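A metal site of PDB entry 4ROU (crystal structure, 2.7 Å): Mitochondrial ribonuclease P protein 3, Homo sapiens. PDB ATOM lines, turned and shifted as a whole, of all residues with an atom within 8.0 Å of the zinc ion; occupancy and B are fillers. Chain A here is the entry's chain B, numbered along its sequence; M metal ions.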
ATOM      1  N   LYS A  63      -4.508  10.708  17.681  1.00  0.00           N
ATOM      2  CA  LYS A  63      -5.793  11.392  17.789  1.00  0.00           C
ATOM      3  C   LYS A  63      -5.617  12.741  18.489  1.00  0.00           C
ATOM      4  O   LYS A  63      -5.109  12.806  19.607  1.00  0.00           O
ATOM      5  CB  LYS A  63      -6.804  10.528  18.535  1.00  0.00           C
ATOM      6  N   GLN A  65      -6.926  16.579  19.950  1.00  0.00           N
ATOM      7  CA  GLN A  65      -8.044  17.303  20.564  1.00  0.00           C
ATOM      8  C   GLN A  65      -7.583  18.627  21.143  1.00  0.00           C
ATOM      9  O   GLN A  65      -6.590  18.690  21.873  1.00  0.00           O
ATOM     10  CB  GLN A  65      -8.705  16.445  21.632  1.00  0.00           C
ATOM     11  N   THR A  67      -7.880  21.324  23.807  1.00  0.00           N
ATOM     12  CA  THR A  67      -8.385  21.268  25.179  1.00  0.00           C
ATOM     13  C   THR A  67      -7.773  22.312  26.111  1.00  0.00           C
ATOM     14  O   THR A  67      -7.104  23.237  25.679  1.00  0.00           O
ATOM     15  CB  THR A  67      -8.137  19.878  25.784  1.00  0.00           C
ATOM     16  OG1 THR A  67      -8.558  19.868  27.158  1.00  0.00           O
ATOM     17  CG2 THR A  67      -6.661  19.527  25.717  1.00  0.00           C
ATOM     18  N   THR A  68      -8.023  22.116  27.407  1.00  0.00           N
ATOM     19  CA  THR A  68      -7.479  22.976  28.450  1.00  0.00           C
ATOM     20  C   THR A  68      -6.887  22.114  29.561  1.00  0.00           C
ATOM     21  O   THR A  68      -6.983  20.888  29.523  1.00  0.00           O
ATOM     22  CB  THR A  68      -8.553  23.914  29.045  1.00  0.00           C
ATOM     23  OG1 THR A  68      -9.624  23.129  29.586  1.00  0.00           O
ATOM     24  CG2 THR A  68      -9.097  24.850  27.974  1.00  0.00           C
ATOM     25  N   VAL A  69      -6.270  22.752  30.547  1.00  0.00           N
ATOM     26  CA  VAL A  69      -5.600  22.031  31.625  1.00  0.00           C
ATOM     27  C   VAL A  69      -6.174  22.382  32.999  1.00  0.00           C
ATOM     28  O   VAL A  69      -6.349  23.562  33.322  1.00  0.00           O
ATOM     29  CB  VAL A  69      -4.084  22.308  31.600  1.00  0.00           C
ATOM     30  CG1 VAL A  69      -3.405  21.644  32.775  1.00  0.00           C
ATOM     31  CG2 VAL A  69      -3.472  21.817  30.298  1.00  0.00           C
ATOM     32  N   GLN A  74      -3.114  16.858  34.727  1.00  0.00           N
ATOM     33  CA  GLN A  74      -4.499  16.452  34.391  1.00  0.00           C
ATOM     34  C   GLN A  74      -5.075  17.197  33.185  1.00  0.00           C
ATOM     35  O   GLN A  74      -5.880  18.118  33.322  1.00  0.00           O
ATOM     36  CB  GLN A  74      -5.455  16.611  35.584  1.00  0.00           C
ATOM     37  CG  GLN A  74      -5.395  15.479  36.597  1.00  0.00           C
ATOM     38  CD  GLN A  74      -6.131  15.813  37.878  1.00  0.00           C
ATOM     39  OE1 GLN A  74      -6.437  16.984  38.135  1.00  0.00           O
ATOM     40  NE2 GLN A  74      -6.423  14.802  38.677  1.00  0.00           N
ATOM     41  N   CYS A  75      -4.654  16.774  31.996  1.00  0.00           N
ATOM     42  CA  CYS A  75      -5.261  17.258  30.763  1.00  0.00           C
ATOM     43  C   CYS A  75      -6.651  16.656  30.597  1.00  0.00           C
ATOM     44  O   CYS A  75      -6.874  15.478  30.877  1.00  0.00           O
ATOM     45  CB  CYS A  75      -4.393  16.904  29.555  1.00  0.00           C
ATOM     46  SG  CYS A  75      -5.231  17.182  27.977  1.00  0.00           S
ATOM     47  N   SER A  76      -7.596  17.490  30.166  1.00  0.00           N
ATOM     48  CA  SER A  76      -8.978  17.070  29.997  1.00  0.00           C
ATOM     49  C   SER A  76      -9.088  15.913  28.991  1.00  0.00           C
ATOM     50  O   SER A  76     -10.012  15.113  29.058  1.00  0.00           O
ATOM     51  CB  SER A  76      -9.846  18.242  29.545  1.00  0.00           C
ATOM     52  OG  SER A  76      -9.883  19.260  30.541  1.00  0.00           O
ATOM     53  N   GLY A  77      -8.132  15.853  28.065  1.00  0.00           N
ATOM     54  CA  GLY A  77      -8.134  14.835  27.027  1.00  0.00           C
ATOM     55  C   GLY A  77      -7.578  13.490  27.462  1.00  0.00           C
ATOM     56  O   GLY A  77      -8.295  12.488  27.421  1.00  0.00           O
ATOM     57  N   CYS A  78      -6.317  13.454  27.873  1.00  0.00           N
ATOM     58  CA  CYS A  78      -5.687  12.196  28.256  1.00  0.00           C
ATOM     59  C   CYS A  78      -6.070  11.745  29.655  1.00  0.00           C
ATOM     60  O   CYS A  78      -6.384  10.579  29.875  1.00  0.00           O
ATOM     61  CB  CYS A  78      -4.155  12.294  28.186  1.00  0.00           C
ATOM     62  SG  CYS A  78      -3.470  13.367  26.930  1.00  0.00           S
ATOM     63  N   GLY A  79      -6.038  12.673  30.594  1.00  0.00           N
ATOM     64  CA  GLY A  79      -6.138  12.348  31.995  1.00  0.00           C
ATOM     65  C   GLY A  79      -4.717  12.296  32.530  1.00  0.00           C
ATOM     66  O   GLY A  79      -4.485  12.240  33.740  1.00  0.00           O
ATOM     67  N   LYS A  80      -3.769  12.296  31.598  1.00  0.00           N
ATOM     68  CA  LYS A  80      -2.343  12.378  31.928  1.00  0.00           C
ATOM     69  C   LYS A  80      -2.039  13.692  32.628  1.00  0.00           C
ATOM     70  O   LYS A  80      -2.706  14.707  32.387  1.00  0.00           O
ATOM     71  CB  LYS A  80      -1.489  12.250  30.670  1.00  0.00           C
ATOM     72  CG  LYS A  80      -1.007  10.841  30.355  1.00  0.00           C
ATOM     73  CD  LYS A  80      -0.127  10.838  29.119  1.00  0.00           C
ATOM     74  CE  LYS A  80       0.631   9.530  28.974  1.00  0.00           C
ATOM     75  NZ  LYS A  80      -0.280   8.360  28.862  1.00  0.00           N
ATOM     76  N   THR A  81      -1.027  13.681  33.485  1.00  0.00           N
ATOM     77  CA  THR A  81      -0.636  14.877  34.218  1.00  0.00           C
ATOM     78  C   THR A  81       0.497  15.614  33.505  1.00  0.00           C
ATOM     79  O   THR A  81       1.564  15.048  33.255  1.00  0.00           O
ATOM     80  CB  THR A  81      -0.214  14.530  35.657  1.00  0.00           C
ATOM     81  OG1 THR A  81      -1.139  13.600  36.218  1.00  0.00           O
ATOM     82  CG2 THR A  81      -0.171  15.789  36.517  1.00  0.00           C
ATOM     83  N   ILE A  82       0.246  16.872  33.170  1.00  0.00           N
ATOM     84  CA  ILE A  82       1.238  17.736  32.551  1.00  0.00           C
ATOM     85  C   ILE A  82       2.494  17.801  33.425  1.00  0.00           C
ATOM     86  O   ILE A  82       2.392  17.732  34.650  1.00  0.00           O
ATOM     87  CB  ILE A  82       0.675  19.160  32.319  1.00  0.00           C
ATOM     88  CG1 ILE A  82      -0.554  19.099  31.409  1.00  0.00           C
ATOM     89  CG2 ILE A  82       1.715  20.099  31.739  1.00  0.00           C
ATOM     90  CD1 ILE A  82      -0.292  18.373  30.100  1.00  0.00           C
ATOM     91  N   SER A 282       2.463  10.396  23.928  1.00  0.00           N
ATOM     92  CA  SER A 282       1.655  11.609  23.984  1.00  0.00           C
ATOM     93  C   SER A 282       2.487  12.870  23.729  1.00  0.00           C
ATOM     94  O   SER A 282       3.675  12.922  24.046  1.00  0.00           O
ATOM     95  CB  SER A 282       0.955  11.720  25.338  1.00  0.00           C
ATOM     96  OG  SER A 282       1.873  12.066  26.356  1.00  0.00           O
ATOM     97  N   TRP A 283       1.840  13.870  23.143  1.00  0.00           N
ATOM     98  CA  TRP A 283       2.404  15.211  23.012  1.00  0.00           C
ATOM     99  C   TRP A 283       1.426  16.226  23.570  1.00  0.00           C
ATOM    100  O   TRP A 283       0.213  16.104  23.375  1.00  0.00           O
ATOM    101  CB  TRP A 283       2.729  15.553  21.561  1.00  0.00           C
ATOM    102  CG  TRP A 283       4.012  14.969  21.039  1.00  0.00           C
ATOM    103  CD1 TRP A 283       4.189  13.722  20.507  1.00  0.00           C
ATOM    104  CD2 TRP A 283       5.279  15.626  20.970  1.00  0.00           C
ATOM    105  NE1 TRP A 283       5.510  13.559  20.131  1.00  0.00           N
ATOM    106  CE2 TRP A 283       6.190  14.714  20.404  1.00  0.00           C
ATOM    107  CE3 TRP A 283       5.743  16.896  21.347  1.00  0.00           C
ATOM    108  CZ2 TRP A 283       7.537  15.025  20.198  1.00  0.00           C
ATOM    109  CZ3 TRP A 283       7.074  17.204  21.145  1.00  0.00           C
ATOM    110  CH2 TRP A 283       7.951  16.277  20.578  1.00  0.00           C
ATOM    111  N   HIS A 284       1.942  17.226  24.285  1.00  0.00           N
ATOM    112  CA  HIS A 284       1.104  18.311  24.762  1.00  0.00           C
ATOM    113  C   HIS A 284       1.691  19.654  24.357  1.00  0.00           C
ATOM    114  O   HIS A 284       2.779  20.026  24.787  1.00  0.00           O
ATOM    115  CB  HIS A 284       0.929  18.236  26.271  1.00  0.00           C
ATOM    116  CG  HIS A 284       0.041  17.118  26.717  1.00  0.00           C
ATOM    117  ND1 HIS A 284       0.482  15.822  26.845  1.00  0.00           N
ATOM    118  CD2 HIS A 284      -1.278  17.093  27.036  1.00  0.00           C
ATOM    119  CE1 HIS A 284      -0.515  15.046  27.239  1.00  0.00           C
ATOM    120  NE2 HIS A 284      -1.594  15.797  27.367  1.00  0.00           N
ATOM    121  N   ILE A 285       0.959  20.373  23.511  1.00  0.00           N
ATOM    122  CA  ILE A 285       1.473  21.583  22.899  1.00  0.00           C
ATOM    123  C   ILE A 285       0.580  22.788  23.184  1.00  0.00           C
ATOM    124  O   ILE A 285      -0.548  22.860  22.692  1.00  0.00           O
ATOM    125  CB  ILE A 285       1.619  21.422  21.378  1.00  0.00           C
ATOM    126  CG1 ILE A 285       2.541  20.250  21.050  1.00  0.00           C
ATOM    127  CG2 ILE A 285       2.139  22.707  20.749  1.00  0.00           C
ATOM    128  CD1 ILE A 285       2.648  19.940  19.575  1.00  0.00           C
ATOM    129  N   TRP A 303      -4.432  24.219  24.784  1.00  0.00           N
ATOM    130  CA  TRP A 303      -3.486  23.135  24.530  1.00  0.00           C
ATOM    131  C   TRP A 303      -3.929  22.235  23.385  1.00  0.00           C
ATOM    132  O   TRP A 303      -5.118  21.955  23.222  1.00  0.00           O
ATOM    133  CB  TRP A 303      -3.300  22.293  25.802  1.00  0.00           C
ATOM    134  CG  TRP A 303      -2.605  23.003  26.915  1.00  0.00           C
ATOM    135  CD1 TRP A 303      -3.100  24.028  27.671  1.00  0.00           C
ATOM    136  CD2 TRP A 303      -1.296  22.725  27.420  1.00  0.00           C
ATOM    137  NE1 TRP A 303      -2.173  24.408  28.615  1.00  0.00           N
ATOM    138  CE2 TRP A 303      -1.050  23.629  28.478  1.00  0.00           C
ATOM    139  CE3 TRP A 303      -0.297  21.808  27.087  1.00  0.00           C
ATOM    140  CZ2 TRP A 303       0.144  23.628  29.200  1.00  0.00           C
ATOM    141  CZ3 TRP A 303       0.889  21.813  27.797  1.00  0.00           C
ATOM    142  CH2 TRP A 303       1.101  22.718  28.840  1.00  0.00           C
ATOM    143  N   LEU A 304      -2.961  21.771  22.605  1.00  0.00           N
ATOM    144  CA  LEU A 304      -3.216  20.709  21.638  1.00  0.00           C
ATOM    145  C   LEU A 304      -2.884  19.361  22.267  1.00  0.00           C
ATOM    146  O   LEU A 304      -1.752  19.110  22.658  1.00  0.00           O
ATOM    147  CB  LEU A 304      -2.409  20.904  20.357  1.00  0.00           C
ATOM    148  CG  LEU A 304      -2.467  19.719  19.384  1.00  0.00           C
ATOM    149  CD1 LEU A 304      -3.902  19.461  18.949  1.00  0.00           C
ATOM    150  CD2 LEU A 304      -1.561  19.945  18.190  1.00  0.00           C
ATOM    151  N   CYS A 305      -3.901  18.501  22.370  1.00  0.00           N
ATOM    152  CA  CYS A 305      -3.738  17.204  23.015  1.00  0.00           C
ATOM    153  C   CYS A 305      -3.573  16.073  21.999  1.00  0.00           C
ATOM    154  O   CYS A 305      -4.438  15.850  21.149  1.00  0.00           O
ATOM    155  CB  CYS A 305      -4.933  16.914  23.918  1.00  0.00           C
ATOM    156  SG  CYS A 305      -4.968  15.262  24.617  1.00  0.00           S
ATOM    157  N   LEU A 306      -2.458  15.352  22.102  1.00  0.00           N
ATOM    158  CA  LEU A 306      -2.190  14.234  21.216  1.00  0.00           C
ATOM    159  C   LEU A 306      -1.798  12.990  22.005  1.00  0.00           C
ATOM    160  O   LEU A 306      -0.945  13.051  22.881  1.00  0.00           O
ATOM    161  CB  LEU A 306      -1.081  14.586  20.222  1.00  0.00           C
ATOM    162  CG  LEU A 306      -1.425  15.663  19.186  1.00  0.00           C
ATOM    163  CD1 LEU A 306      -0.161  16.354  18.690  1.00  0.00           C
ATOM    164  CD2 LEU A 306      -2.180  15.057  18.019  1.00  0.00           C
ATOM    165  N   HIS A 307      -2.436  11.864  21.695  1.00  0.00           N
ATOM    166  CA  HIS A 307      -2.136  10.611  22.388  1.00  0.00           C
ATOM    167  C   HIS A 307      -2.276   9.417  21.447  1.00  0.00           C
ATOM    168  O   HIS A 307      -3.260   9.310  20.709  1.00  0.00           O
ATOM    169  CB  HIS A 307      -3.058  10.437  23.592  1.00  0.00           C
HETATM  170 ZN    ZN M   1      -4.044  15.581  26.858  1.00  0.00          ZN
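Within 4 Å of the zinc ion: Cys 75, Cys 78, His 284 and Cys 305.
The zinc ion is bound by SG of Cys 75, SG of Cys 78, SG of Cys 305 and NE2 of His 284. The zinc ion has four donor atoms within binding distance.
The backbone NH of Gly 77 lies close to the side-chain sulfur of Cys 75 (3.2 Å). N of Cys 75 sits at hydrogen-bond distance from O of Lys 80 (2.9 Å). N of Cys 305 sits at hydrogen-bond distance from O of Gln 65.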
